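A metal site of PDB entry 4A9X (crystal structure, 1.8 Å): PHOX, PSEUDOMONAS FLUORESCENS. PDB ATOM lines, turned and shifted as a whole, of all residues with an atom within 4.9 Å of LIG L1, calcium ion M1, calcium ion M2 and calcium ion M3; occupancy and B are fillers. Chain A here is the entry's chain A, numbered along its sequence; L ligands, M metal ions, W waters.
Residues that only touch calcium ion M2: Cys 179 and Trp 388.
Five residues have an atom within 4 Å of calcium ion M2: Cys 179, Glu 273, Glu 387, Trp 388 and Asp 479.
The nearest printed residue that does not touch calcium ion M2 is Glu 532 (4.2 Å).
An iron atom (FE2) of LG2 L2 is bound by an oxygen (O3) of LIG L1, 2.1 Å away.
Arg 385 touches calcium ion M1.
The side-chain carboxylate (OE2) of Glu 90 sits close to an oxygen (O2) of LIG L1 (3.2 Å).
OE2 of Glu 194 lies close to O3 of LIG L1 (2.9 Å).
The side-chain carboxylate of Asp 292 lies close to an oxygen (O3) of LIG L1.
Within 4 Å of LIG L1: Glu 90, Glu 194, Asn 195, Arg 223, Asp 292, Arg 294, Arg 385, Glu 387, Asp 479, Asp 494 and Glu 532.
The nearest printed residue that does not touch LIG L1 is Glu 273 (4.1 Å).
Within 4 Å of calcium ion M3: Asp 494 and Glu 532.
The nearest printed residue that does not touch calcium ion M3 is Gln 550 (4.4 Å).
The backbone carbonyl oxygen (O) of Asp 479 lies within hydrogen-bond range of the backbone NH (N) of Trp 388 (3.2 Å).
The backbone NH (N) of Gln 550 sits at hydrogen-bond distance from the backbone carbonyl oxygen (O) of Glu 532, at 3.0 Å.
The side-chain carboxylate (OE1) of Glu 532 sits close to a ring nitrogen (NE2) of His 551.
The side-chain carboxylate (OE2) of Glu 273 lies close to the indole nitrogen (NE1) of Trp 388 (3.2 Å).
The guanidinium group of Arg 385 lies within salt-bridge range of the side-chain carboxylate of Asp 292, 2.8 Å away.
The side-chain carboxylate of Glu 387 lies close to the guanidinium group of Arg 385 (3.8 Å).
O of Arg 385 is in hydrogen-bond range of N of Thr 403, at 3.2 Å.
The side-chain amide nitrogen of Asn 195 sits close to the side-chain carboxylate of Glu 194.
The guanidinium group (NE) of Arg 385 sits at hydrogen-bond distance from an oxygen (O11) of LIG L1 (3.3 Å).
N5 of LIG L1 lies close to NH1 of Arg 223, 3.4 Å away.
NH1 of Arg 294 is in hydrogen-bond range of O10 of LIG L1 (3.3 Å).
OD1 of Asn 195 sits at hydrogen-bond distance from O12 of LIG L1, at 3.3 Å.
OE1 of Glu 273 is bound to FE2 of LG2 L2.
The side-chain carboxylate (OD2) of Asp 292 is bound to an iron atom (FE2) of LG2 L2, at 2.0 Å.
The side-chain carboxylate of Glu 387 binds an iron atom (FE2) of LG2 L2 (2.2 Å).
OE2 of Glu 194 binds FE2 of LG2 L2.
The side-chain carboxylate (OE2) of Glu 90 is bound to an iron atom (FE1) of LG2 L2 (2.1 Å).
The side-chain sulfur (SG) of Cys 179 binds an iron atom (FE1) of LG2 L2.
Calcium ion M1 is bound by the side-chain carboxylate (OD2) of Asp 494, the side-chain carboxylate (OD2) of Asp 479, an oxygen (O1) of LIG L1, water W5, an oxygen (O4) of LIG L1, the side-chain carboxylate (OE1) of Glu 387 and the side-chain carboxylate (OE2) of Glu 387.
Calcium ion M3 is bound by OE1 of Glu 532 (2.3 Å), OD2 of Asp 494 (2.4 Å), water W13 (2.4 Å), O1 of LIG L1 (2.5 Å), water W6 (2.5 Å), water W14 (2.5 Å) and O5 of LIG L1 (2.7 Å).
Calcium ion M3 has seven donor atoms within binding distance.
Slightly farther from calcium ion M3 lies the side-chain carboxylate (OE2) of Glu 532 (3.0 Å).
O1 of LG2 L2 is bound to calcium ion M2.
OE2 of Glu 273 is bound to calcium ion M2.
Calcium ion M2 is bound by OD1 of Asp 479 (2.4 Å).
OD2 of Asp 479 binds calcium ion M2.
Calcium ion M2 is bound by water W3, 2.6 Å away.
Calcium ion M2 is bound by water W15 (2.8 Å).
Water W1 is bound to calcium ion M2, 2.8 Å away.
Slightly farther from calcium ion M2 lies OE1 of Glu 387 (3.1 Å).
Water W3 lies within hydrogen-bond range of the side-chain carboxylate of Glu 532 (2.6 Å) and the side-chain hydroxyl of Thr 534 (2.7 Å).
Water W15 bridges OD2 of Asp 69 (2.5 Å) and OE1 of Glu 90 (3.2 Å).
Water W1 lies within hydrogen-bond range of the side-chain carboxylate of Asp 69 (2.5 Å), the indole nitrogen of Trp 388 (2.7 Å) and the side-chain hydroxyl of Thr 534 (3.4 Å).
Water W4 lies within hydrogen-bond range of OD1 of Asn 195 (2.5 Å), O12 of LIG L1 (2.8 Å) and O of Asp 292 (2.9 Å).
Water W10 lies within hydrogen-bond range of an oxygen (O11) of LIG L1 (2.8 Å) and the backbone NH (N) of Arg 294 (3.0 Å).
Water W7 lies within hydrogen-bond range of the guanidinium group of Arg 223 and an oxygen (O12) of LIG L1.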
ATOM      1  N   ASP A  69     -12.827   5.516  15.351  1.00  0.00           N
ATOM      2  CA  ASP A  69     -14.239   5.821  15.537  1.00  0.00           C
ATOM      3  C   ASP A  69     -14.677   5.434  16.957  1.00  0.00           C
ATOM      4  O   ASP A  69     -14.136   5.986  17.919  1.00  0.00           O
ATOM      5  CB  ASP A  69     -14.992   5.149  14.360  1.00  0.00           C
ATOM      6  CG  ASP A  69     -16.346   5.708  13.945  1.00  0.00           C
ATOM      7  OD1 ASP A  69     -17.075   6.218  14.798  1.00  0.00           O
ATOM      8  OD2 ASP A  69     -16.726   5.522  12.775  1.00  0.00           O
ATOM      9  N   GLU A  90     -12.658   2.466  11.247  1.00  0.00           N
ATOM     10  CA  GLU A  90     -13.759   2.287  10.306  1.00  0.00           C
ATOM     11  C   GLU A  90     -13.386   2.105   8.870  1.00  0.00           C
ATOM     12  O   GLU A  90     -13.826   1.155   8.227  1.00  0.00           O
ATOM     13  CB  GLU A  90     -14.789   3.431  10.447  1.00  0.00           C
ATOM     14  CG  GLU A  90     -16.090   3.213   9.688  1.00  0.00           C
ATOM     15  CD  GLU A  90     -17.071   4.353   9.894  1.00  0.00           C
ATOM     16  OE1 GLU A  90     -16.632   5.524   9.824  1.00  0.00           O
ATOM     17  OE2 GLU A  90     -18.242   4.067  10.201  1.00  0.00           O
ATOM     18  N   CYS A 179     -17.678   0.736  13.016  1.00  0.00           N
ATOM     19  CA  CYS A 179     -18.210   2.062  13.269  1.00  0.00           C
ATOM     20  C   CYS A 179     -18.136   2.346  14.775  1.00  0.00           C
ATOM     21  O   CYS A 179     -17.068   2.785  15.216  1.00  0.00           O
ATOM     22  CB  CYS A 179     -19.620   2.152  12.696  1.00  0.00           C
ATOM     23  SG  CYS A 179     -20.446   3.716  12.991  1.00  0.00           S
ATOM     24  N   GLU A 194     -20.739  -1.680  10.199  1.00  0.00           N
ATOM     25  CA  GLU A 194     -21.737  -0.803   9.647  1.00  0.00           C
ATOM     26  C   GLU A 194     -21.849  -0.885   8.112  1.00  0.00           C
ATOM     27  O   GLU A 194     -22.608  -1.712   7.641  1.00  0.00           O
ATOM     28  CB  GLU A 194     -21.507   0.612  10.142  1.00  0.00           C
ATOM     29  CG  GLU A 194     -22.625   1.640   9.861  1.00  0.00           C
ATOM     30  CD  GLU A 194     -22.199   3.101   9.917  1.00  0.00           C
ATOM     31  OE1 GLU A 194     -20.991   3.358   9.775  1.00  0.00           O
ATOM     32  OE2 GLU A 194     -23.067   3.979  10.104  1.00  0.00           O
ATOM     33  N   ASN A 195     -21.100  -0.066   7.341  1.00  0.00           N
ATOM     34  CA  ASN A 195     -21.197  -0.064   5.868  1.00  0.00           C
ATOM     35  C   ASN A 195     -20.279  -1.097   5.178  1.00  0.00           C
ATOM     36  O   ASN A 195     -19.622  -0.806   4.180  1.00  0.00           O
ATOM     37  CB  ASN A 195     -20.985   1.340   5.338  1.00  0.00           C
ATOM     38  CG  ASN A 195     -22.105   2.280   5.701  1.00  0.00           C
ATOM     39  OD1 ASN A 195     -23.232   2.121   5.236  1.00  0.00           O
ATOM     40  ND2 ASN A 195     -21.838   3.316   6.484  1.00  0.00           N
ATOM     41  N   ARG A 223     -18.978   0.509  -3.650  1.00  0.00           N
ATOM     42  CA  ARG A 223     -19.224   1.935  -3.398  1.00  0.00           C
ATOM     43  C   ARG A 223     -17.873   2.652  -3.334  1.00  0.00           C
ATOM     44  O   ARG A 223     -17.478   3.186  -2.294  1.00  0.00           O
ATOM     45  CB  ARG A 223     -20.090   2.124  -2.140  1.00  0.00           C
ATOM     46  CG  ARG A 223     -20.716   3.502  -2.025  1.00  0.00           C
ATOM     47  CD  ARG A 223     -21.743   3.592  -0.913  1.00  0.00           C
ATOM     48  NE  ARG A 223     -22.973   2.862  -1.236  1.00  0.00           N
ATOM     49  CZ  ARG A 223     -23.989   2.655  -0.398  1.00  0.00           C
ATOM     50  NH1 ARG A 223     -23.940   3.136   0.844  1.00  0.00           N
ATOM     51  NH2 ARG A 223     -25.063   1.988  -0.791  1.00  0.00           N
ATOM     52  N   GLU A 273     -24.417   0.502  13.873  1.00  0.00           N
ATOM     53  CA  GLU A 273     -23.713   1.701  14.282  1.00  0.00           C
ATOM     54  C   GLU A 273     -23.063   1.409  15.662  1.00  0.00           C
ATOM     55  O   GLU A 273     -21.874   1.224  15.686  1.00  0.00           O
ATOM     56  CB  GLU A 273     -24.653   2.894  14.355  1.00  0.00           C
ATOM     57  CG  GLU A 273     -23.948   4.150  14.821  1.00  0.00           C
ATOM     58  CD  GLU A 273     -23.448   5.048  13.717  1.00  0.00           C
ATOM     59  OE1 GLU A 273     -23.991   4.991  12.592  1.00  0.00           O
ATOM     60  OE2 GLU A 273     -22.563   5.881  14.003  1.00  0.00           O
ATOM     61  N   ASP A 292     -27.881   2.119  10.639  1.00  0.00           N
ATOM     62  CA  ASP A 292     -27.698   3.451  10.059  1.00  0.00           C
ATOM     63  C   ASP A 292     -27.823   3.457   8.550  1.00  0.00           C
ATOM     64  O   ASP A 292     -26.858   3.287   7.805  1.00  0.00           O
ATOM     65  CB  ASP A 292     -26.377   4.102  10.495  1.00  0.00           C
ATOM     66  CG  ASP A 292     -26.179   5.480   9.879  1.00  0.00           C
ATOM     67  OD1 ASP A 292     -27.168   6.043   9.371  1.00  0.00           O
ATOM     68  OD2 ASP A 292     -25.049   5.980   9.892  1.00  0.00           O
ATOM     69  N   GLU A 293     -29.051   3.666   8.110  1.00  0.00           N
ATOM     70  CA  GLU A 293     -29.388   3.845   6.701  1.00  0.00           C
ATOM     71  C   GLU A 293     -30.762   4.508   6.671  1.00  0.00           C
ATOM     72  O   GLU A 293     -31.623   4.210   7.514  1.00  0.00           O
ATOM     73  CB  GLU A 293     -29.325   2.512   5.928  1.00  0.00           C
ATOM     74  CG  GLU A 293     -29.780   2.598   4.479  1.00  0.00           C
ATOM     75  CD  GLU A 293     -29.438   1.428   3.570  1.00  0.00           C
ATOM     76  OE1 GLU A 293     -28.634   0.564   3.973  1.00  0.00           O
ATOM     77  OE2 GLU A 293     -30.016   1.348   2.454  1.00  0.00           O
ATOM     78  N   ARG A 294     -30.950   5.428   5.721  1.00  0.00           N
ATOM     79  CA  ARG A 294     -32.224   6.149   5.555  1.00  0.00           C
ATOM     80  C   ARG A 294     -33.407   5.170   5.515  1.00  0.00           C
ATOM     81  O   ARG A 294     -33.407   4.248   4.730  1.00  0.00           O
ATOM     82  CB  ARG A 294     -32.207   6.968   4.254  1.00  0.00           C
ATOM     83  CG  ARG A 294     -31.403   8.250   4.345  1.00  0.00           C
ATOM     84  CD  ARG A 294     -31.485   9.018   3.038  1.00  0.00           C
ATOM     85  NE  ARG A 294     -30.707   8.378   1.959  1.00  0.00           N
ATOM     86  CZ  ARG A 294     -29.431   8.626   1.663  1.00  0.00           C
ATOM     87  NH1 ARG A 294     -28.739   9.521   2.367  1.00  0.00           N
ATOM     88  NH2 ARG A 294     -28.841   7.986   0.661  1.00  0.00           N
ATOM     89  N   ARG A 385     -32.152   7.646   9.930  1.00  0.00           N
ATOM     90  CA  ARG A 385     -30.774   7.219  10.150  1.00  0.00           C
ATOM     91  C   ARG A 385     -30.391   7.090  11.625  1.00  0.00           C
ATOM     92  O   ARG A 385     -29.668   7.926  12.158  1.00  0.00           O
ATOM     93  CB  ARG A 385     -29.790   8.132   9.430  1.00  0.00           C
ATOM     94  CG  ARG A 385     -29.812   7.985   7.921  1.00  0.00           C
ATOM     95  CD  ARG A 385     -28.691   8.742   7.271  1.00  0.00           C
ATOM     96  NE  ARG A 385     -27.406   8.266   7.729  1.00  0.00           N
ATOM     97  CZ  ARG A 385     -26.259   8.940   7.642  1.00  0.00           C
ATOM     98  NH1 ARG A 385     -26.244  10.169   7.133  1.00  0.00           N
ATOM     99  NH2 ARG A 385     -25.129   8.403   8.089  1.00  0.00           N
ATOM    100  N   GLU A 387     -28.219   6.526  14.536  1.00  0.00           N
ATOM    101  CA  GLU A 387     -26.781   6.365  14.725  1.00  0.00           C
ATOM    102  C   GLU A 387     -26.516   5.905  16.167  1.00  0.00           C
ATOM    103  O   GLU A 387     -26.940   4.792  16.460  1.00  0.00           O
ATOM    104  CB  GLU A 387     -25.947   7.573  14.237  1.00  0.00           C
ATOM    105  CG  GLU A 387     -25.965   7.685  12.713  1.00  0.00           C
ATOM    106  CD  GLU A 387     -24.788   8.413  12.074  1.00  0.00           C
ATOM    107  OE1 GLU A 387     -23.852   7.769  11.562  1.00  0.00           O
ATOM    108  OE2 GLU A 387     -24.828   9.665  12.087  1.00  0.00           O
ATOM    109  N   TRP A 388     -25.846   6.677  17.051  1.00  0.00           N
ATOM    110  CA  TRP A 388     -25.538   6.130  18.362  1.00  0.00           C
ATOM    111  C   TRP A 388     -26.691   6.131  19.325  1.00  0.00           C
ATOM    112  O   TRP A 388     -27.519   7.044  19.341  1.00  0.00           O
ATOM    113  CB  TRP A 388     -24.374   6.842  19.035  1.00  0.00           C
ATOM    114  CG  TRP A 388     -23.028   6.664  18.392  1.00  0.00           C
ATOM    115  CD1 TRP A 388     -22.746   6.729  17.071  1.00  0.00           C
ATOM    116  CD2 TRP A 388     -21.764   6.685  19.070  1.00  0.00           C
ATOM    117  NE1 TRP A 388     -21.382   6.698  16.878  1.00  0.00           N
ATOM    118  CE2 TRP A 388     -20.764   6.785  18.087  1.00  0.00           C
ATOM    119  CE3 TRP A 388     -21.391   6.686  20.418  1.00  0.00           C
ATOM    120  CZ2 TRP A 388     -19.388   6.789  18.413  1.00  0.00           C
ATOM    121  CZ3 TRP A 388     -20.038   6.757  20.742  1.00  0.00           C
ATOM    122  CH2 TRP A 388     -19.058   6.731  19.746  1.00  0.00           C
ATOM    123  N   THR A 403     -29.524  11.098  12.517  1.00  0.00           N
ATOM    124  CA  THR A 403     -28.571  12.075  12.010  1.00  0.00           C
ATOM    125  C   THR A 403     -29.114  12.982  10.942  1.00  0.00           C
ATOM    126  O   THR A 403     -28.841  14.175  10.960  1.00  0.00           O
ATOM    127  CB  THR A 403     -27.230  11.422  11.644  1.00  0.00           C
ATOM    128  OG1 THR A 403     -26.203  12.391  11.767  1.00  0.00           O
ATOM    129  CG2 THR A 403     -27.191  10.802  10.230  1.00  0.00           C
ATOM    130  N   ASP A 479     -24.370  12.560  15.724  1.00  0.00           N
ATOM    131  CA  ASP A 479     -24.055  11.163  15.418  1.00  0.00           C
ATOM    132  C   ASP A 479     -23.674  10.421  16.712  1.00  0.00           C
ATOM    133  O   ASP A 479     -24.465   9.609  17.199  1.00  0.00           O
ATOM    134  CB  ASP A 479     -22.966  11.195  14.336  1.00  0.00           C
ATOM    135  CG  ASP A 479     -22.384   9.895  13.804  1.00  0.00           C
ATOM    136  OD1 ASP A 479     -22.536   8.866  14.475  1.00  0.00           O
ATOM    137  OD2 ASP A 479     -21.852   9.911  12.678  1.00  0.00           O
ATOM    138  N   ASP A 494     -21.341  14.878  12.999  1.00  0.00           N
ATOM    139  CA  ASP A 494     -20.782  14.405  11.755  1.00  0.00           C
ATOM    140  C   ASP A 494     -21.667  14.948  10.651  1.00  0.00           C
ATOM    141  O   ASP A 494     -22.452  14.211  10.041  1.00  0.00           O
ATOM    142  CB  ASP A 494     -20.747  12.890  11.713  1.00  0.00           C
ATOM    143  CG  ASP A 494     -20.418  12.383  10.327  1.00  0.00           C
ATOM    144  OD1 ASP A 494     -19.797  13.157   9.539  1.00  0.00           O
ATOM    145  OD2 ASP A 494     -20.811  11.241  10.024  1.00  0.00           O
ATOM    146  N   GLU A 532     -14.650  14.701  11.342  1.00  0.00           N
ATOM    147  CA  GLU A 532     -15.865  14.507  12.099  1.00  0.00           C
ATOM    148  C   GLU A 532     -15.387  14.136  13.516  1.00  0.00           C
ATOM    149  O   GLU A 532     -14.252  13.671  13.693  1.00  0.00           O
ATOM    150  CB  GLU A 532     -16.812  13.476  11.481  1.00  0.00           C
ATOM    151  CG  GLU A 532     -16.562  12.032  11.871  1.00  0.00           C
ATOM    152  CD  GLU A 532     -17.438  11.044  11.124  1.00  0.00           C
ATOM    153  OE1 GLU A 532     -17.388  11.079   9.876  1.00  0.00           O
ATOM    154  OE2 GLU A 532     -18.212  10.304  11.783  1.00  0.00           O
ATOM    155  N   THR A 534     -15.929  11.864  16.627  1.00  0.00           N
ATOM    156  CA  THR A 534     -16.525  10.569  16.954  1.00  0.00           C
ATOM    157  C   THR A 534     -15.684   9.831  17.950  1.00  0.00           C
ATOM    158  O   THR A 534     -14.489  10.079  18.048  1.00  0.00           O
ATOM    159  CB  THR A 534     -16.760   9.804  15.646  1.00  0.00           C
ATOM    160  OG1 THR A 534     -17.455   8.588  15.914  1.00  0.00           O
ATOM    161  CG2 THR A 534     -15.463   9.581  14.865  1.00  0.00           C
ATOM    162  N   GLN A 550     -11.773  12.032  13.369  1.00  0.00           N
ATOM    163  CA  GLN A 550     -11.728  11.131  12.247  1.00  0.00           C
ATOM    164  C   GLN A 550     -11.655  11.883  10.937  1.00  0.00           C
ATOM    165  O   GLN A 550     -12.307  12.930  10.780  1.00  0.00           O
ATOM    166  CB  GLN A 550     -12.998  10.267  12.287  1.00  0.00           C
ATOM    167  CG  GLN A 550     -12.935   9.067  11.377  1.00  0.00           C
ATOM    168  CD  GLN A 550     -14.268   8.432  11.182  1.00  0.00           C
ATOM    169  OE1 GLN A 550     -15.223   9.071  10.781  1.00  0.00           O
ATOM    170  NE2 GLN A 550     -14.371   7.136  11.445  1.00  0.00           N
ATOM    171  N   HIS A 551     -10.824  11.363  10.023  1.00  0.00           N
ATOM    172  CA  HIS A 551     -10.549  11.842   8.652  1.00  0.00           C
ATOM    173  C   HIS A 551     -10.315  13.347   8.525  1.00  0.00           C
ATOM    174  O   HIS A 551     -10.910  14.035   7.689  1.00  0.00           O
ATOM    175  CB  HIS A 551     -11.576  11.342   7.609  1.00  0.00           C
ATOM    176  CG  HIS A 551     -13.000  11.719   7.887  1.00  0.00           C
ATOM    177  ND1 HIS A 551     -13.432  13.019   7.753  1.00  0.00           N
ATOM    178  CD2 HIS A 551     -14.018  10.976   8.374  1.00  0.00           C
ATOM    179  CE1 HIS A 551     -14.707  13.017   8.108  1.00  0.00           C
ATOM    180  NE2 HIS A 551     -15.100  11.818   8.495  1.00  0.00           N
HETATM  181  P1  LIG L   1     -21.267   7.266   8.769  1.00  0.00           P
HETATM  182  O1  LIG L   1     -21.013   8.407   9.698  1.00  0.00           O
HETATM  183  O2  LIG L   1     -20.157   6.192   8.848  1.00  0.00           O
HETATM  184  O3  LIG L   1     -22.648   6.614   9.023  1.00  0.00           O
HETATM  185  P2  LIG L   1     -21.770   9.395   6.998  1.00  0.00           P
HETATM  186  O4  LIG L   1     -22.849   9.870   7.974  1.00  0.00           O
HETATM  187  O5  LIG L   1     -20.557  10.346   6.716  1.00  0.00           O
HETATM  188  C1  LIG L   1     -21.334   7.778   7.139  1.00  0.00           C
HETATM  189  P3  LIG L   1     -22.191   9.894   4.125  1.00  0.00           P
HETATM  190  O6  LIG L   1     -21.048   9.074   3.661  1.00  0.00           O
HETATM  191  O7  LIG L   1     -22.197  11.379   3.822  1.00  0.00           O
HETATM  192  O8  LIG L   1     -22.597   9.700   5.671  1.00  0.00           O
HETATM  193  O9  LIG L   1     -23.609   9.508   3.334  1.00  0.00           O
HETATM  194  C2  LIG L   1     -24.940   9.697   3.863  1.00  0.00           C
HETATM  195  C3  LIG L   1     -25.652   8.374   3.985  1.00  0.00           C
HETATM  196  O10 LIG L   1     -25.907   7.836   2.666  1.00  0.00           O
HETATM  197  C4  LIG L   1     -24.962   7.255   4.762  1.00  0.00           C
HETATM  198  O11 LIG L   1     -25.943   6.430   5.401  1.00  0.00           O
HETATM  199  C5  LIG L   1     -24.245   6.472   3.673  1.00  0.00           C
HETATM  200  O12 LIG L   1     -24.047   5.114   4.041  1.00  0.00           O
HETATM  201  C6  LIG L   1     -25.247   6.591   2.508  1.00  0.00           C
HETATM  202  N1  LIG L   1     -24.657   6.574   1.177  1.00  0.00           N
HETATM  203  C7  LIG L   1     -23.471   7.128   0.786  1.00  0.00           C
HETATM  204  N2  LIG L   1     -23.208   6.998  -0.495  1.00  0.00           N
HETATM  205  C8  LIG L   1     -24.316   6.307  -0.983  1.00  0.00           C
HETATM  206  C9  LIG L   1     -24.651   5.845  -2.272  1.00  0.00           C
HETATM  207  N3  LIG L   1     -23.835   5.910  -3.322  1.00  0.00           N
HETATM  208  N4  LIG L   1     -25.830   5.202  -2.417  1.00  0.00           N
HETATM  209  C10 LIG L   1     -26.600   5.006  -1.341  1.00  0.00           C
HETATM  210  N5  LIG L   1     -26.377   5.385  -0.070  1.00  0.00           N
HETATM  211  C11 LIG L   1     -25.220   6.040   0.038  1.00  0.00           C
HETATM  212 FE1  LG2 L   2     -20.051   4.918  10.834  1.00  0.00          FE
HETATM  213 FE2  LG2 L   2     -23.302   5.793  10.876  1.00  0.00          FE
HETATM  214  O1  LG2 L   2     -21.494   6.056  11.429  1.00  0.00           O
HETATM  215 CA    CA M   1     -22.626   9.899  10.493  1.00  0.00          CA
HETATM  216 CA    CA M   2     -21.181   7.530  13.022  1.00  0.00          CA
HETATM  217 CA    CA M   3     -19.156   9.849   8.995  1.00  0.00          CA
HETATM  218  O   HOH W   1     -19.590   6.106  14.889  1.00  0.00           O
HETATM  219  O   HOH W   2     -19.143   4.427   7.169  1.00  0.00           O
HETATM  220  O   HOH W   3     -19.169   8.971  13.850  1.00  0.00           O
HETATM  221  O   HOH W   4     -25.509   3.104   5.258  1.00  0.00           O
HETATM  222  O   HOH W   5     -24.024  11.984  10.330  1.00  0.00           O
HETATM  223  O   HOH W   6     -18.743  11.855   7.601  1.00  0.00           O
HETATM  224  O   HOH W   7     -21.896   4.305   2.348  1.00  0.00           O
HETATM  225  O   HOH W   8     -24.300  12.476   7.377  1.00  0.00           O
HETATM  226  O   HOH W   9     -18.579   8.725   4.757  1.00  0.00           O
HETATM  227  O   HOH W  10     -28.439   6.157   4.199  1.00  0.00           O
HETATM  228  O   HOH W  11     -24.203   5.320   7.067  1.00  0.00           O
HETATM  229  O   HOH W  12     -28.183   4.745   1.843  1.00  0.00           O
HETATM  230  O   HOH W  13     -17.746   9.720   7.012  1.00  0.00           O
HETATM  231  O   HOH W  14     -17.583   7.988   9.741  1.00  0.00           O
HETATM  232  O   HOH W  15     -18.835   6.534  11.884  1.00  0.00           O
